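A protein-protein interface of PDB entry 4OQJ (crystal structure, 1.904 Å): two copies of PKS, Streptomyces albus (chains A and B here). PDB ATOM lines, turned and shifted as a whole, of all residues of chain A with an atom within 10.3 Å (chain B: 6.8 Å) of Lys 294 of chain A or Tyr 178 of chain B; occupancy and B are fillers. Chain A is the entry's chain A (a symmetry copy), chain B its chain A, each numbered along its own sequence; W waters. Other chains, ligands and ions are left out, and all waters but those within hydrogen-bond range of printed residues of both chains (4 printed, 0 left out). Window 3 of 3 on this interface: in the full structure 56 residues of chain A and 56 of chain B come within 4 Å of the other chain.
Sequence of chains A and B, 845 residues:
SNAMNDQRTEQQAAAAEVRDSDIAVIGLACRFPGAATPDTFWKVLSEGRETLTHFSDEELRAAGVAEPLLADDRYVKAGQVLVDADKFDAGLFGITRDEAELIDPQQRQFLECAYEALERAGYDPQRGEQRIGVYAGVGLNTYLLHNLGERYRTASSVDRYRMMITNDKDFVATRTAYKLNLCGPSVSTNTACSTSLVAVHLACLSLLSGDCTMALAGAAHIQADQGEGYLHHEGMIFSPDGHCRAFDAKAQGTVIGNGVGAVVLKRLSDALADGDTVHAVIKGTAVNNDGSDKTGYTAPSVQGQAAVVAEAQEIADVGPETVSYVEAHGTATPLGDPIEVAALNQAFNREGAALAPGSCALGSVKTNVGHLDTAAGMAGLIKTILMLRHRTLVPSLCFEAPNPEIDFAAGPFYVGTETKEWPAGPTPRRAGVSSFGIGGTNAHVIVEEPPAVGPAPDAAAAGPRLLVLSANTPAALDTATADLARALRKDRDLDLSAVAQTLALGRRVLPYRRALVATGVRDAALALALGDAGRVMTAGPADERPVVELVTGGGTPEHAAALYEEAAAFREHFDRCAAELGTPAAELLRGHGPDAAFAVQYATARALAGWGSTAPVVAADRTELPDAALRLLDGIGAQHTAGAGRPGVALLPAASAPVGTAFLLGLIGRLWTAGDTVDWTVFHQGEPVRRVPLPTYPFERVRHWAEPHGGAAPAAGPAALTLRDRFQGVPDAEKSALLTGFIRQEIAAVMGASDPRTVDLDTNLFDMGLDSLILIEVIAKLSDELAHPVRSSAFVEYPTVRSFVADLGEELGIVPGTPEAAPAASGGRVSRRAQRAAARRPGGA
Asn 289 of chain A touches Ala 177 of chain B. OG of Ser 186 of chain B touches CB of Asn 289 of chain A, at 3.5 Å. O of Ala 177 of chain B touches CA of Gly 291 of chain A (3.7 Å). Gly 291 of chain A touches Asn 181 of chain B (CA to OD1, 3.6 Å). O of Lys 294 of chain A touches OH of Tyr 178 of chain B, at 3.9 Å. Gly 439 of chain A touches Thr 174 of chain B. CG2 of Thr 174 of chain B touches OG1 of Thr 441 of chain A (3.5 Å).
Lys 294 of chain A touches just one residue of chain B: Tyr 178 (3.9 Å). Of chain A, only Gly 291, Ser 292, Lys 294, Gly 296 and Tyr 297 come within 4 Å of Tyr 178 of chain B. Of chain A, only Asn 289 (3.5 Å) and Gly 291 (3.7 Å) come within 4 Å of Ala 177 of chain B. No residue of chain A comes within 4 Å of Lys 179 of chain B. Of the printed residues of chain A, Thr 174 of chain B touches Tyr 297 (2.6 Å), Gly 439 (3.3 Å) and Thr 441 (3.5 Å). Of the printed residues of chain A, Asn 181 of chain B touches Gly 291 (3.6 Å) and Ser 292 (2.8 Å). Printed residues of chain A within 4 Å of Leu 182 of chain B: Asn 289 and Gly 291. Pro 300 of chain A touches none of the printed residues of chain B. The nearest printed residue of chain B that does not touch Lys 294 of chain A is Asn 181 of chain B (7.3 Å).
No position is printed for both chains.
The side-chain amide nitrogen (ND2) of Asn 289 of chain A lies within hydrogen-bond range of the backbone carbonyl oxygen (O) of Gly 439 of chain A (3.0 Å). The side-chain amide nitrogen of Asn 289 of chain A is in hydrogen-bond range of the side-chain hydroxyl of Thr 441 of chain A. The side-chain amino group of Lys 294 of chain A sits at hydrogen-bond distance from the backbone carbonyl oxygen of Ala 299 of chain A (2.9 Å).
The side-chain hydroxyl (OH) of Tyr 297 of chain A lies within hydrogen-bond range of the side-chain hydroxyl (OG1) of Thr 174 of chain B. OH of Tyr 297 of chain A lies within hydrogen-bond range of N of Arg 175 of chain B (3.3 Å). The backbone carbonyl oxygen (O) of Tyr 178 of chain B lies within hydrogen-bond range of the side-chain hydroxyl (OG) of Ser 292 of chain A (2.6 Å). OH of Tyr 178 of chain B lies close to N of Gly 296 of chain A (3.4 Å). OH of Tyr 178 of chain B lies close to N of Tyr 297 of chain A. The side-chain amide oxygen (OD1) of Asn 181 of chain B is in hydrogen-bond range of the backbone NH (N) of Ser 292 of chain A (2.8 Å). The backbone carbonyl oxygen (O) of Ser 186 of chain B sits at hydrogen-bond distance from the side-chain hydroxyl (OG1) of Thr 441 of chain A (2.8 Å).
Water W3 bridges the side-chain hydroxyl (OG) of Ser 292 of chain A (2.7 Å) and the backbone carbonyl oxygen (O) of Lys 179 of chain B (3.0 Å). Water W1 bridges O of Ile 438 of chain A (2.8 Å) and OG1 of Thr 174 of chain B (2.8 Å). Water W4 lies within hydrogen-bond range of O of Thr 295 of chain A and OH of Tyr 178 of chain B.
Of the 12 printed residues of chain B, 7 touch a printed residue of chain A. Hydrophobic or aromatic side chains of chain B within 4 Å of the printed part of chain A: Ala 177 and Tyr 178. Of the 26 printed residues of chain A, 8 touch a printed residue of chain B. Hydrophobic or aromatic side chains of chain A that line the printed part of chain B: Tyr 297. Among the printed residues, 17 pairs touch across the chains. Among the printed residues, no Asp or Glu carboxylate lies within 4 Å of a Lys or Arg side-chain nitrogen of the other chain.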
ATOM      1  N   ASN A 288       6.317 -14.546 -28.327  1.00  0.00           N
ATOM      2  CA  ASN A 288       6.342 -13.399 -27.454  1.00  0.00           C
ATOM      3  C   ASN A 288       5.142 -13.458 -26.505  1.00  0.00           C
ATOM      4  O   ASN A 288       4.394 -14.446 -26.497  1.00  0.00           O
ATOM      5  CB  ASN A 288       6.377 -12.091 -28.271  1.00  0.00           C
ATOM      6  CG  ASN A 288       5.059 -11.781 -28.966  1.00  0.00           C
ATOM      7  OD1 ASN A 288       4.049 -12.415 -28.710  1.00  0.00           O
ATOM      8  ND2 ASN A 288       5.066 -10.773 -29.845  1.00  0.00           N
ATOM      9  N   ASN A 289       4.990 -12.441 -25.675  1.00  0.00           N
ATOM     10  CA  ASN A 289       3.776 -12.303 -24.873  1.00  0.00           C
ATOM     11  C   ASN A 289       3.263 -10.885 -25.003  1.00  0.00           C
ATOM     12  O   ASN A 289       4.053  -9.936 -25.151  1.00  0.00           O
ATOM     13  CB  ASN A 289       4.025 -12.664 -23.405  1.00  0.00           C
ATOM     14  CG  ASN A 289       2.744 -12.717 -22.590  1.00  0.00           C
ATOM     15  OD1 ASN A 289       2.210 -11.679 -22.162  1.00  0.00           O
ATOM     16  ND2 ASN A 289       2.235 -13.922 -22.380  1.00  0.00           N
ATOM     17  N   ASP A 290       1.943 -10.733 -24.933  1.00  0.00           N
ATOM     18  CA  ASP A 290       1.304  -9.414 -25.006  1.00  0.00           C
ATOM     19  C   ASP A 290       1.742  -8.464 -23.898  1.00  0.00           C
ATOM     20  O   ASP A 290       1.730  -7.235 -24.071  1.00  0.00           O
ATOM     21  CB  ASP A 290      -0.214  -9.558 -24.935  1.00  0.00           C
ATOM     22  CG  ASP A 290      -0.789 -10.274 -26.132  1.00  0.00           C
ATOM     23  OD1 ASP A 290      -0.141 -10.250 -27.196  1.00  0.00           O
ATOM     24  OD2 ASP A 290      -1.882 -10.855 -26.000  1.00  0.00           O
ATOM     25  N   GLY A 291       2.100  -9.022 -22.744  1.00  0.00           N
ATOM     26  CA  GLY A 291       2.402  -8.195 -21.598  1.00  0.00           C
ATOM     27  C   GLY A 291       1.121  -7.552 -21.096  1.00  0.00           C
ATOM     28  O   GLY A 291       0.041  -8.140 -21.222  1.00  0.00           O
ATOM     29  N   SER A 292       1.233  -6.352 -20.541  1.00  0.00           N
ATOM     30  CA  SER A 292       0.135  -5.740 -19.805  1.00  0.00           C
ATOM     31  C   SER A 292      -0.784  -4.884 -20.670  1.00  0.00           C
ATOM     32  O   SER A 292      -1.903  -4.582 -20.265  1.00  0.00           O
ATOM     33  CB  SER A 292       0.676  -4.857 -18.668  1.00  0.00           C
ATOM     34  OG  SER A 292       1.327  -5.649 -17.680  1.00  0.00           O
ATOM     35  N   ASP A 293      -0.312  -4.470 -21.837  1.00  0.00           N
ATOM     36  CA  ASP A 293      -0.983  -3.371 -22.555  1.00  0.00           C
ATOM     37  C   ASP A 293      -2.164  -3.895 -23.392  1.00  0.00           C
ATOM     38  O   ASP A 293      -2.090  -4.037 -24.615  1.00  0.00           O
ATOM     39  CB  ASP A 293       0.028  -2.632 -23.426  1.00  0.00           C
ATOM     40  CG  ASP A 293      -0.555  -1.393 -24.084  1.00  0.00           C
ATOM     41  OD1 ASP A 293      -1.636  -0.928 -23.651  1.00  0.00           O
ATOM     42  OD2 ASP A 293       0.082  -0.882 -25.031  1.00  0.00           O
ATOM     43  N   LYS A 294      -3.240  -4.220 -22.695  1.00  0.00           N
ATOM     44  CA  LYS A 294      -4.458  -4.720 -23.311  1.00  0.00           C
ATOM     45  C   LYS A 294      -5.505  -4.756 -22.201  1.00  0.00           C
ATOM     46  O   LYS A 294      -5.164  -4.613 -21.031  1.00  0.00           O
ATOM     47  CB  LYS A 294      -4.248  -6.085 -23.958  1.00  0.00           C
ATOM     48  CG  LYS A 294      -3.961  -7.238 -23.005  1.00  0.00           C
ATOM     49  CD  LYS A 294      -3.744  -8.504 -23.816  1.00  0.00           C
ATOM     50  CE  LYS A 294      -3.720  -9.750 -22.981  1.00  0.00           C
ATOM     51  NZ  LYS A 294      -3.569 -10.966 -23.848  1.00  0.00           N
ATOM     52  N   THR A 295      -6.768  -4.940 -22.565  1.00  0.00           N
ATOM     53  CA  THR A 295      -7.881  -4.642 -21.673  1.00  0.00           C
ATOM     54  C   THR A 295      -8.210  -5.715 -20.643  1.00  0.00           C
ATOM     55  O   THR A 295      -9.059  -5.503 -19.779  1.00  0.00           O
ATOM     56  CB  THR A 295      -9.167  -4.385 -22.483  1.00  0.00           C
ATOM     57  OG1 THR A 295      -9.531  -5.577 -23.197  1.00  0.00           O
ATOM     58  CG2 THR A 295      -8.963  -3.238 -23.464  1.00  0.00           C
ATOM     59  N   GLY A 296      -7.549  -6.857 -20.719  1.00  0.00           N
ATOM     60  CA  GLY A 296      -7.810  -7.927 -19.777  1.00  0.00           C
ATOM     61  C   GLY A 296      -6.935  -9.127 -20.061  1.00  0.00           C
ATOM     62  O   GLY A 296      -6.463  -9.288 -21.172  1.00  0.00           O
ATOM     63  N   TYR A 297      -6.739  -9.969 -19.051  1.00  0.00           N
ATOM     64  CA  TYR A 297      -5.911 -11.161 -19.170  1.00  0.00           C
ATOM     65  C   TYR A 297      -6.282 -12.017 -20.380  1.00  0.00           C
ATOM     66  O   TYR A 297      -5.404 -12.550 -21.072  1.00  0.00           O
ATOM     67  CB  TYR A 297      -6.026 -11.990 -17.881  1.00  0.00           C
ATOM     68  CG  TYR A 297      -5.112 -13.195 -17.801  1.00  0.00           C
ATOM     69  CD1 TYR A 297      -3.743 -13.078 -18.037  1.00  0.00           C
ATOM     70  CD2 TYR A 297      -5.609 -14.440 -17.450  1.00  0.00           C
ATOM     71  CE1 TYR A 297      -2.899 -14.168 -17.936  1.00  0.00           C
ATOM     72  CE2 TYR A 297      -4.779 -15.535 -17.344  1.00  0.00           C
ATOM     73  CZ  TYR A 297      -3.421 -15.401 -17.576  1.00  0.00           C
ATOM     74  OH  TYR A 297      -2.596 -16.508 -17.482  1.00  0.00           O
ATOM     75  N   THR A 298      -7.581 -12.162 -20.627  1.00  0.00           N
ATOM     76  CA  THR A 298      -8.059 -13.005 -21.720  1.00  0.00           C
ATOM     77  C   THR A 298      -8.296 -12.249 -23.039  1.00  0.00           C
ATOM     78  O   THR A 298      -8.643 -12.867 -24.041  1.00  0.00           O
ATOM     79  CB  THR A 298      -9.373 -13.697 -21.350  1.00  0.00           C
ATOM     80  OG1 THR A 298     -10.290 -12.709 -20.860  1.00  0.00           O
ATOM     81  CG2 THR A 298      -9.134 -14.777 -20.294  1.00  0.00           C
ATOM     82  N   ALA A 299      -8.113 -10.932 -23.031  1.00  0.00           N
ATOM     83  CA  ALA A 299      -8.334 -10.110 -24.218  1.00  0.00           C
ATOM     84  C   ALA A 299      -7.315 -10.399 -25.324  1.00  0.00           C
ATOM     85  O   ALA A 299      -6.212 -10.858 -25.041  1.00  0.00           O
ATOM     86  CB  ALA A 299      -8.272  -8.655 -23.847  1.00  0.00           C
ATOM     87  N   PRO A 300      -7.673 -10.107 -26.591  1.00  0.00           N
ATOM     88  CA  PRO A 300      -6.701 -10.228 -27.679  1.00  0.00           C
ATOM     89  C   PRO A 300      -5.796  -8.996 -27.757  1.00  0.00           C
ATOM     90  O   PRO A 300      -6.034  -8.024 -27.042  1.00  0.00           O
ATOM     91  CB  PRO A 300      -7.580 -10.345 -28.933  1.00  0.00           C
ATOM     92  CG  PRO A 300      -9.008 -10.162 -28.467  1.00  0.00           C
ATOM     93  CD  PRO A 300      -8.958  -9.601 -27.092  1.00  0.00           C
ATOM     94  N   SER A 301      -4.769  -9.045 -28.603  1.00  0.00           N
ATOM     95  CA  SER A 301      -3.853  -7.915 -28.758  1.00  0.00           C
ATOM     96  C   SER A 301      -3.309  -7.823 -30.188  1.00  0.00           C
ATOM     97  O   SER A 301      -2.533  -8.692 -30.634  1.00  0.00           O
ATOM     98  CB  SER A 301      -2.696  -8.045 -27.753  1.00  0.00           C
ATOM     99  OG  SER A 301      -1.671  -7.080 -27.979  1.00  0.00           O
ATOM    100  N   VAL A 302      -3.706  -6.771 -30.903  1.00  0.00           N
ATOM    101  CA  VAL A 302      -3.221  -6.547 -32.265  1.00  0.00           C
ATOM    102  C   VAL A 302      -1.701  -6.462 -32.268  1.00  0.00           C
ATOM    103  O   VAL A 302      -1.035  -7.074 -33.093  1.00  0.00           O
ATOM    104  CB  VAL A 302      -3.779  -5.248 -32.892  1.00  0.00           C
ATOM    105  CG1 VAL A 302      -3.330  -5.120 -34.347  1.00  0.00           C
ATOM    106  CG2 VAL A 302      -5.284  -5.214 -32.837  1.00  0.00           C
ATOM    107  N   GLN A 303      -1.156  -5.702 -31.327  1.00  0.00           N
ATOM    108  CA  GLN A 303       0.278  -5.433 -31.349  1.00  0.00           C
ATOM    109  C   GLN A 303       1.113  -6.659 -31.055  1.00  0.00           C
ATOM    110  O   GLN A 303       2.133  -6.869 -31.711  1.00  0.00           O
ATOM    111  CB  GLN A 303       0.609  -4.305 -30.379  1.00  0.00           C
ATOM    112  CG  GLN A 303       0.053  -2.971 -30.857  1.00  0.00           C
ATOM    113  CD  GLN A 303       0.409  -2.675 -32.326  1.00  0.00           C
ATOM    114  OE1 GLN A 303       1.548  -2.878 -32.757  1.00  0.00           O
ATOM    115  NE2 GLN A 303      -0.577  -2.216 -33.096  1.00  0.00           N
ATOM    116  N   GLY A 304       0.679  -7.481 -30.100  1.00  0.00           N
ATOM    117  CA  GLY A 304       1.393  -8.700 -29.773  1.00  0.00           C
ATOM    118  C   GLY A 304       1.429  -9.650 -30.956  1.00  0.00           C
ATOM    119  O   GLY A 304       2.467 -10.236 -31.280  1.00  0.00           O
ATOM    120  N   GLN A 305       0.285  -9.819 -31.601  1.00  0.00           N
ATOM    121  CA  GLN A 305       0.195 -10.671 -32.786  1.00  0.00           C
ATOM    122  C   GLN A 305       1.046 -10.113 -33.936  1.00  0.00           C
ATOM    123  O   GLN A 305       1.834 -10.837 -34.552  1.00  0.00           O
ATOM    124  CB  GLN A 305      -1.254 -10.807 -33.250  1.00  0.00           C
ATOM    125  CG  GLN A 305      -2.189 -11.558 -32.312  1.00  0.00           C
ATOM    126  CD  GLN A 305      -3.605 -11.653 -32.896  1.00  0.00           C
ATOM    127  OE1 GLN A 305      -3.785 -11.631 -34.109  1.00  0.00           O
ATOM    128  NE2 GLN A 305      -4.602 -11.730 -32.033  1.00  0.00           N
ATOM    129  N   ILE A 339      -9.263  -8.423 -35.606  1.00  0.00           N
ATOM    130  CA  ILE A 339      -7.985  -8.168 -34.956  1.00  0.00           C
ATOM    131  C   ILE A 339      -6.873  -9.013 -35.594  1.00  0.00           C
ATOM    132  O   ILE A 339      -5.770  -8.510 -35.855  1.00  0.00           O
ATOM    133  CB  ILE A 339      -8.086  -8.436 -33.419  1.00  0.00           C
ATOM    134  CG1 ILE A 339      -8.812  -7.251 -32.750  1.00  0.00           C
ATOM    135  CG2 ILE A 339      -6.717  -8.668 -32.794  1.00  0.00           C
ATOM    136  CD1 ILE A 339      -8.890  -7.309 -31.250  1.00  0.00           C
ATOM    137  N   PHE A 436      -2.273 -18.239 -30.943  1.00  0.00           N
ATOM    138  CA  PHE A 436      -2.302 -17.253 -29.863  1.00  0.00           C
ATOM    139  C   PHE A 436      -3.050 -17.782 -28.644  1.00  0.00           C
ATOM    140  O   PHE A 436      -4.216 -18.147 -28.730  1.00  0.00           O
ATOM    141  CB  PHE A 436      -2.962 -15.960 -30.336  1.00  0.00           C
ATOM    142  CG  PHE A 436      -2.446 -15.475 -31.650  1.00  0.00           C
ATOM    143  CD1 PHE A 436      -1.086 -15.393 -31.886  1.00  0.00           C
ATOM    144  CD2 PHE A 436      -3.318 -15.119 -32.664  1.00  0.00           C
ATOM    145  CE1 PHE A 436      -0.610 -14.937 -33.105  1.00  0.00           C
ATOM    146  CE2 PHE A 436      -2.840 -14.671 -33.891  1.00  0.00           C
ATOM    147  CZ  PHE A 436      -1.500 -14.581 -34.107  1.00  0.00           C
ATOM    148  N   GLY A 437      -2.370 -17.833 -27.506  1.00  0.00           N
ATOM    149  CA  GLY A 437      -2.949 -18.423 -26.309  1.00  0.00           C
ATOM    150  C   GLY A 437      -3.685 -17.481 -25.370  1.00  0.00           C
ATOM    151  O   GLY A 437      -3.386 -16.292 -25.289  1.00  0.00           O
ATOM    152  N   ILE A 438      -4.653 -18.026 -24.638  1.00  0.00           N
ATOM    153  CA  ILE A 438      -5.160 -17.356 -23.448  1.00  0.00           C
ATOM    154  C   ILE A 438      -3.970 -17.125 -22.522  1.00  0.00           C
ATOM    155  O   ILE A 438      -3.203 -18.040 -22.276  1.00  0.00           O
ATOM    156  CB  ILE A 438      -6.236 -18.186 -22.729  1.00  0.00           C
ATOM    157  CG1 ILE A 438      -7.458 -18.348 -23.630  1.00  0.00           C
ATOM    158  CG2 ILE A 438      -6.635 -17.532 -21.413  1.00  0.00           C
ATOM    159  CD1 ILE A 438      -8.148 -17.028 -23.995  1.00  0.00           C
ATOM    160  N   GLY A 439      -3.817 -15.900 -22.043  1.00  0.00           N
ATOM    161  CA  GLY A 439      -2.675 -15.520 -21.230  1.00  0.00           C
ATOM    162  C   GLY A 439      -1.639 -14.764 -22.043  1.00  0.00           C
ATOM    163  O   GLY A 439      -0.652 -14.229 -21.501  1.00  0.00           O
ATOM    164  N   GLY A 440      -1.847 -14.747 -23.356  1.00  0.00           N
ATOM    165  CA  GLY A 440      -1.160 -13.816 -24.231  1.00  0.00           C
ATOM    166  C   GLY A 440       0.174 -14.249 -24.804  1.00  0.00           C
ATOM    167  O   GLY A 440       0.884 -13.415 -25.362  1.00  0.00           O
ATOM    168  N   THR A 441       0.534 -15.522 -24.685  1.00  0.00           N
ATOM    169  CA  THR A 441       1.764 -15.970 -25.333  1.00  0.00           C
ATOM    170  C   THR A 441       1.428 -16.341 -26.774  1.00  0.00           C
ATOM    171  O   THR A 441       0.577 -17.197 -27.029  1.00  0.00           O
ATOM    172  CB  THR A 441       2.426 -17.126 -24.581  1.00  0.00           C
ATOM    173  OG1 THR A 441       3.061 -16.594 -23.415  1.00  0.00           O
ATOM    174  CG2 THR A 441       3.496 -17.816 -25.446  1.00  0.00           C
ATOM    175  N   ASN A 442       2.093 -15.646 -27.700  1.00  0.00           N
ATOM    176  CA  ASN A 442       1.862 -15.763 -29.130  1.00  0.00           C
ATOM    177  C   ASN A 442       2.995 -16.474 -29.820  1.00  0.00           C
ATOM    178  O   ASN A 442       4.136 -16.310 -29.441  1.00  0.00           O
ATOM    179  CB  ASN A 442       1.715 -14.386 -29.755  1.00  0.00           C
ATOM    180  CG  ASN A 442       0.702 -13.527 -29.036  1.00  0.00           C
ATOM    181  OD1 ASN A 442      -0.427 -13.945 -28.837  1.00  0.00           O
ATOM    182  ND2 ASN A 442       1.106 -12.310 -28.638  1.00  0.00           N
ATOM    183  N   PHE B  93      -2.043  -6.019  -7.503  1.00  0.00           N
ATOM    184  CA  PHE B  93      -2.063  -6.623  -8.831  1.00  0.00           C
ATOM    185  C   PHE B  93      -3.421  -6.484  -9.538  1.00  0.00           C
ATOM    186  O   PHE B  93      -3.643  -7.071 -10.591  1.00  0.00           O
ATOM    187  CB  PHE B  93      -1.663  -8.092  -8.723  1.00  0.00           C
ATOM    188  CG  PHE B  93      -0.264  -8.283  -8.246  1.00  0.00           C
ATOM    189  CD1 PHE B  93       0.806  -7.914  -9.046  1.00  0.00           C
ATOM    190  CD2 PHE B  93      -0.006  -8.789  -6.983  1.00  0.00           C
ATOM    191  CE1 PHE B  93       2.113  -8.075  -8.604  1.00  0.00           C
ATOM    192  CE2 PHE B  93       1.295  -8.939  -6.539  1.00  0.00           C
ATOM    193  CZ  PHE B  93       2.353  -8.584  -7.357  1.00  0.00           C
ATOM    194  N   ALA B 173       3.225 -18.668 -15.790  1.00  0.00           N
ATOM    195  CA  ALA B 173       4.152 -17.779 -16.460  1.00  0.00           C
ATOM    196  C   ALA B 173       3.396 -16.642 -17.119  1.00  0.00           C
ATOM    197  O   ALA B 173       3.839 -15.506 -17.053  1.00  0.00           O
ATOM    198  CB  ALA B 173       5.002 -18.539 -17.495  1.00  0.00           C
ATOM    199  N   THR B 174       2.264 -16.935 -17.757  1.00  0.00           N
ATOM    200  CA  THR B 174       1.526 -15.891 -18.451  1.00  0.00           C
ATOM    201  C   THR B 174       0.790 -14.916 -17.505  1.00  0.00           C
ATOM    202  O   THR B 174       0.669 -13.741 -17.820  1.00  0.00           O
ATOM    203  CB  THR B 174       0.502 -16.494 -19.421  1.00  0.00           C
ATOM    204  OG1 THR B 174      -0.420 -17.317 -18.694  1.00  0.00           O
ATOM    205  CG2 THR B 174       1.219 -17.303 -20.495  1.00  0.00           C
ATOM    206  N   ARG B 175       0.291 -15.397 -16.372  1.00  0.00           N
ATOM    207  CA  ARG B 175      -0.267 -14.494 -15.358  1.00  0.00           C
ATOM    208  C   ARG B 175       0.787 -13.491 -14.938  1.00  0.00           C
ATOM    209  O   ARG B 175       0.509 -12.292 -14.836  1.00  0.00           O
ATOM    210  CB  ARG B 175      -0.757 -15.249 -14.130  1.00  0.00           C
ATOM    211  CG  ARG B 175      -1.341 -14.324 -13.040  1.00  0.00           C
ATOM    212  CD  ARG B 175      -1.799 -15.093 -11.825  1.00  0.00           C
ATOM    213  NE  ARG B 175      -2.242 -16.408 -12.215  1.00  0.00           N
ATOM    214  CZ  ARG B 175      -3.404 -16.657 -12.803  1.00  0.00           C
ATOM    215  NH1 ARG B 175      -3.690 -17.890 -13.175  1.00  0.00           N
ATOM    216  NH2 ARG B 175      -4.270 -15.682 -13.023  1.00  0.00           N
ATOM    217  N   THR B 176       2.005 -13.979 -14.733  1.00  0.00           N
ATOM    218  CA  THR B 176       3.105 -13.110 -14.345  1.00  0.00           C
ATOM    219  C   THR B 176       3.418 -12.127 -15.465  1.00  0.00           C
ATOM    220  O   THR B 176       3.628 -10.944 -15.204  1.00  0.00           O
ATOM    221  CB  THR B 176       4.353 -13.941 -13.968  1.00  0.00           C
ATOM    222  OG1 THR B 176       4.008 -14.826 -12.890  1.00  0.00           O
ATOM    223  CG2 THR B 176       5.496 -13.064 -13.530  1.00  0.00           C
ATOM    224  N   ALA B 177       3.435 -12.601 -16.710  1.00  0.00           N
ATOM    225  CA  ALA B 177       3.731 -11.709 -17.838  1.00  0.00           C
ATOM    226  C   ALA B 177       2.673 -10.608 -17.932  1.00  0.00           C
ATOM    227  O   ALA B 177       2.990  -9.431 -18.153  1.00  0.00           O
ATOM    228  CB  ALA B 177       3.800 -12.492 -19.121  1.00  0.00           C
ATOM    229  N   TYR B 178       1.413 -10.982 -17.751  1.00  0.00           N
ATOM    230  CA  TYR B 178       0.318 -10.029 -17.865  1.00  0.00           C
ATOM    231  C   TYR B 178       0.324  -8.996 -16.736  1.00  0.00           C
ATOM    232  O   TYR B 178       0.048  -7.812 -16.954  1.00  0.00           O
ATOM    233  CB  TYR B 178      -1.026 -10.760 -17.875  1.00  0.00           C
ATOM    234  CG  TYR B 178      -2.190  -9.809 -17.910  1.00  0.00           C
ATOM    235  CD1 TYR B 178      -2.415  -9.020 -19.033  1.00  0.00           C
ATOM    236  CD2 TYR B 178      -3.055  -9.677 -16.821  1.00  0.00           C
ATOM    237  CE1 TYR B 178      -3.466  -8.125 -19.087  1.00  0.00           C
ATOM    238  CE2 TYR B 178      -4.131  -8.774 -16.864  1.00  0.00           C
ATOM    239  CZ  TYR B 178      -4.317  -8.001 -18.008  1.00  0.00           C
ATOM    240  OH  TYR B 178      -5.344  -7.095 -18.091  1.00  0.00           O
ATOM    241  N   LYS B 179       0.644  -9.433 -15.528  1.00  0.00           N
ATOM    242  CA  LYS B 179       0.549  -8.542 -14.380  1.00  0.00           C
ATOM    243  C   LYS B 179       1.811  -7.726 -14.156  1.00  0.00           C
ATOM    244  O   LYS B 179       1.738  -6.666 -13.541  1.00  0.00           O
ATOM    245  CB  LYS B 179       0.228  -9.341 -13.125  1.00  0.00           C
ATOM    246  CG  LYS B 179      -1.179  -9.892 -13.094  1.00  0.00           C
ATOM    247  CD  LYS B 179      -2.204  -8.780 -13.029  1.00  0.00           C
ATOM    248  CE  LYS B 179      -3.593  -9.355 -12.922  1.00  0.00           C
ATOM    249  NZ  LYS B 179      -4.599  -8.275 -12.811  1.00  0.00           N
ATOM    250  N   LEU B 180       2.960  -8.217 -14.632  1.00  0.00           N
ATOM    251  CA  LEU B 180       4.231  -7.488 -14.496  1.00  0.00           C
ATOM    252  C   LEU B 180       4.682  -6.768 -15.781  1.00  0.00           C
ATOM    253  O   LEU B 180       5.619  -5.982 -15.743  1.00  0.00           O
ATOM    254  CB  LEU B 180       5.344  -8.434 -14.050  1.00  0.00           C
ATOM    255  CG  LEU B 180       5.131  -9.176 -12.722  1.00  0.00           C
ATOM    256  CD1 LEU B 180       6.434  -9.818 -12.266  1.00  0.00           C
ATOM    257  CD2 LEU B 180       4.596  -8.247 -11.647  1.00  0.00           C
ATOM    258  N   ASN B 181       4.010  -7.048 -16.899  1.00  0.00           N
ATOM    259  CA  ASN B 181       4.356  -6.552 -18.254  1.00  0.00           C
ATOM    260  C   ASN B 181       5.641  -7.153 -18.831  1.00  0.00           C
ATOM    261  O   ASN B 181       6.578  -6.439 -19.191  1.00  0.00           O
ATOM    262  CB  ASN B 181       4.475  -5.025 -18.300  1.00  0.00           C
ATOM    263  CG  ASN B 181       4.429  -4.489 -19.735  1.00  0.00           C
ATOM    264  OD1 ASN B 181       3.653  -4.972 -20.560  1.00  0.00           O
ATOM    265  ND2 ASN B 181       5.265  -3.502 -20.041  1.00  0.00           N
ATOM    266  N   LEU B 182       5.661  -8.473 -18.960  1.00  0.00           N
ATOM    267  CA  LEU B 182       6.790  -9.180 -19.554  1.00  0.00           C
ATOM    268  C   LEU B 182       6.349  -9.572 -20.956  1.00  0.00           C
ATOM    269  O   LEU B 182       5.363 -10.300 -21.103  1.00  0.00           O
ATOM    270  CB  LEU B 182       7.169 -10.405 -18.712  1.00  0.00           C
ATOM    271  CG  LEU B 182       7.268 -10.178 -17.208  1.00  0.00           C
ATOM    272  CD1 LEU B 182       7.740 -11.425 -16.503  1.00  0.00           C
ATOM    273  CD2 LEU B 182       8.192  -8.994 -16.891  1.00  0.00           C
ATOM    274  N   SER B 186       6.836 -16.268 -22.654  1.00  0.00           N
ATOM    275  CA  SER B 186       6.371 -16.586 -21.322  1.00  0.00           C
ATOM    276  C   SER B 186       5.812 -17.994 -21.350  1.00  0.00           C
ATOM    277  O   SER B 186       4.776 -18.263 -21.970  1.00  0.00           O
ATOM    278  CB  SER B 186       5.338 -15.556 -20.870  1.00  0.00           C
ATOM    279  OG  SER B 186       5.931 -14.248 -20.903  1.00  0.00           O
HETATM  280  O   HOH W   1      -1.357 -19.167 -20.564  1.00  0.00           O
HETATM  281  O   HOH W   2       2.486  -4.838 -22.989  1.00  0.00           O
HETATM  282  O   HOH W   3       1.849  -4.305 -15.416  1.00  0.00           O
HETATM  283  O   HOH W   4      -7.002  -4.076 -17.540  1.00  0.00           O
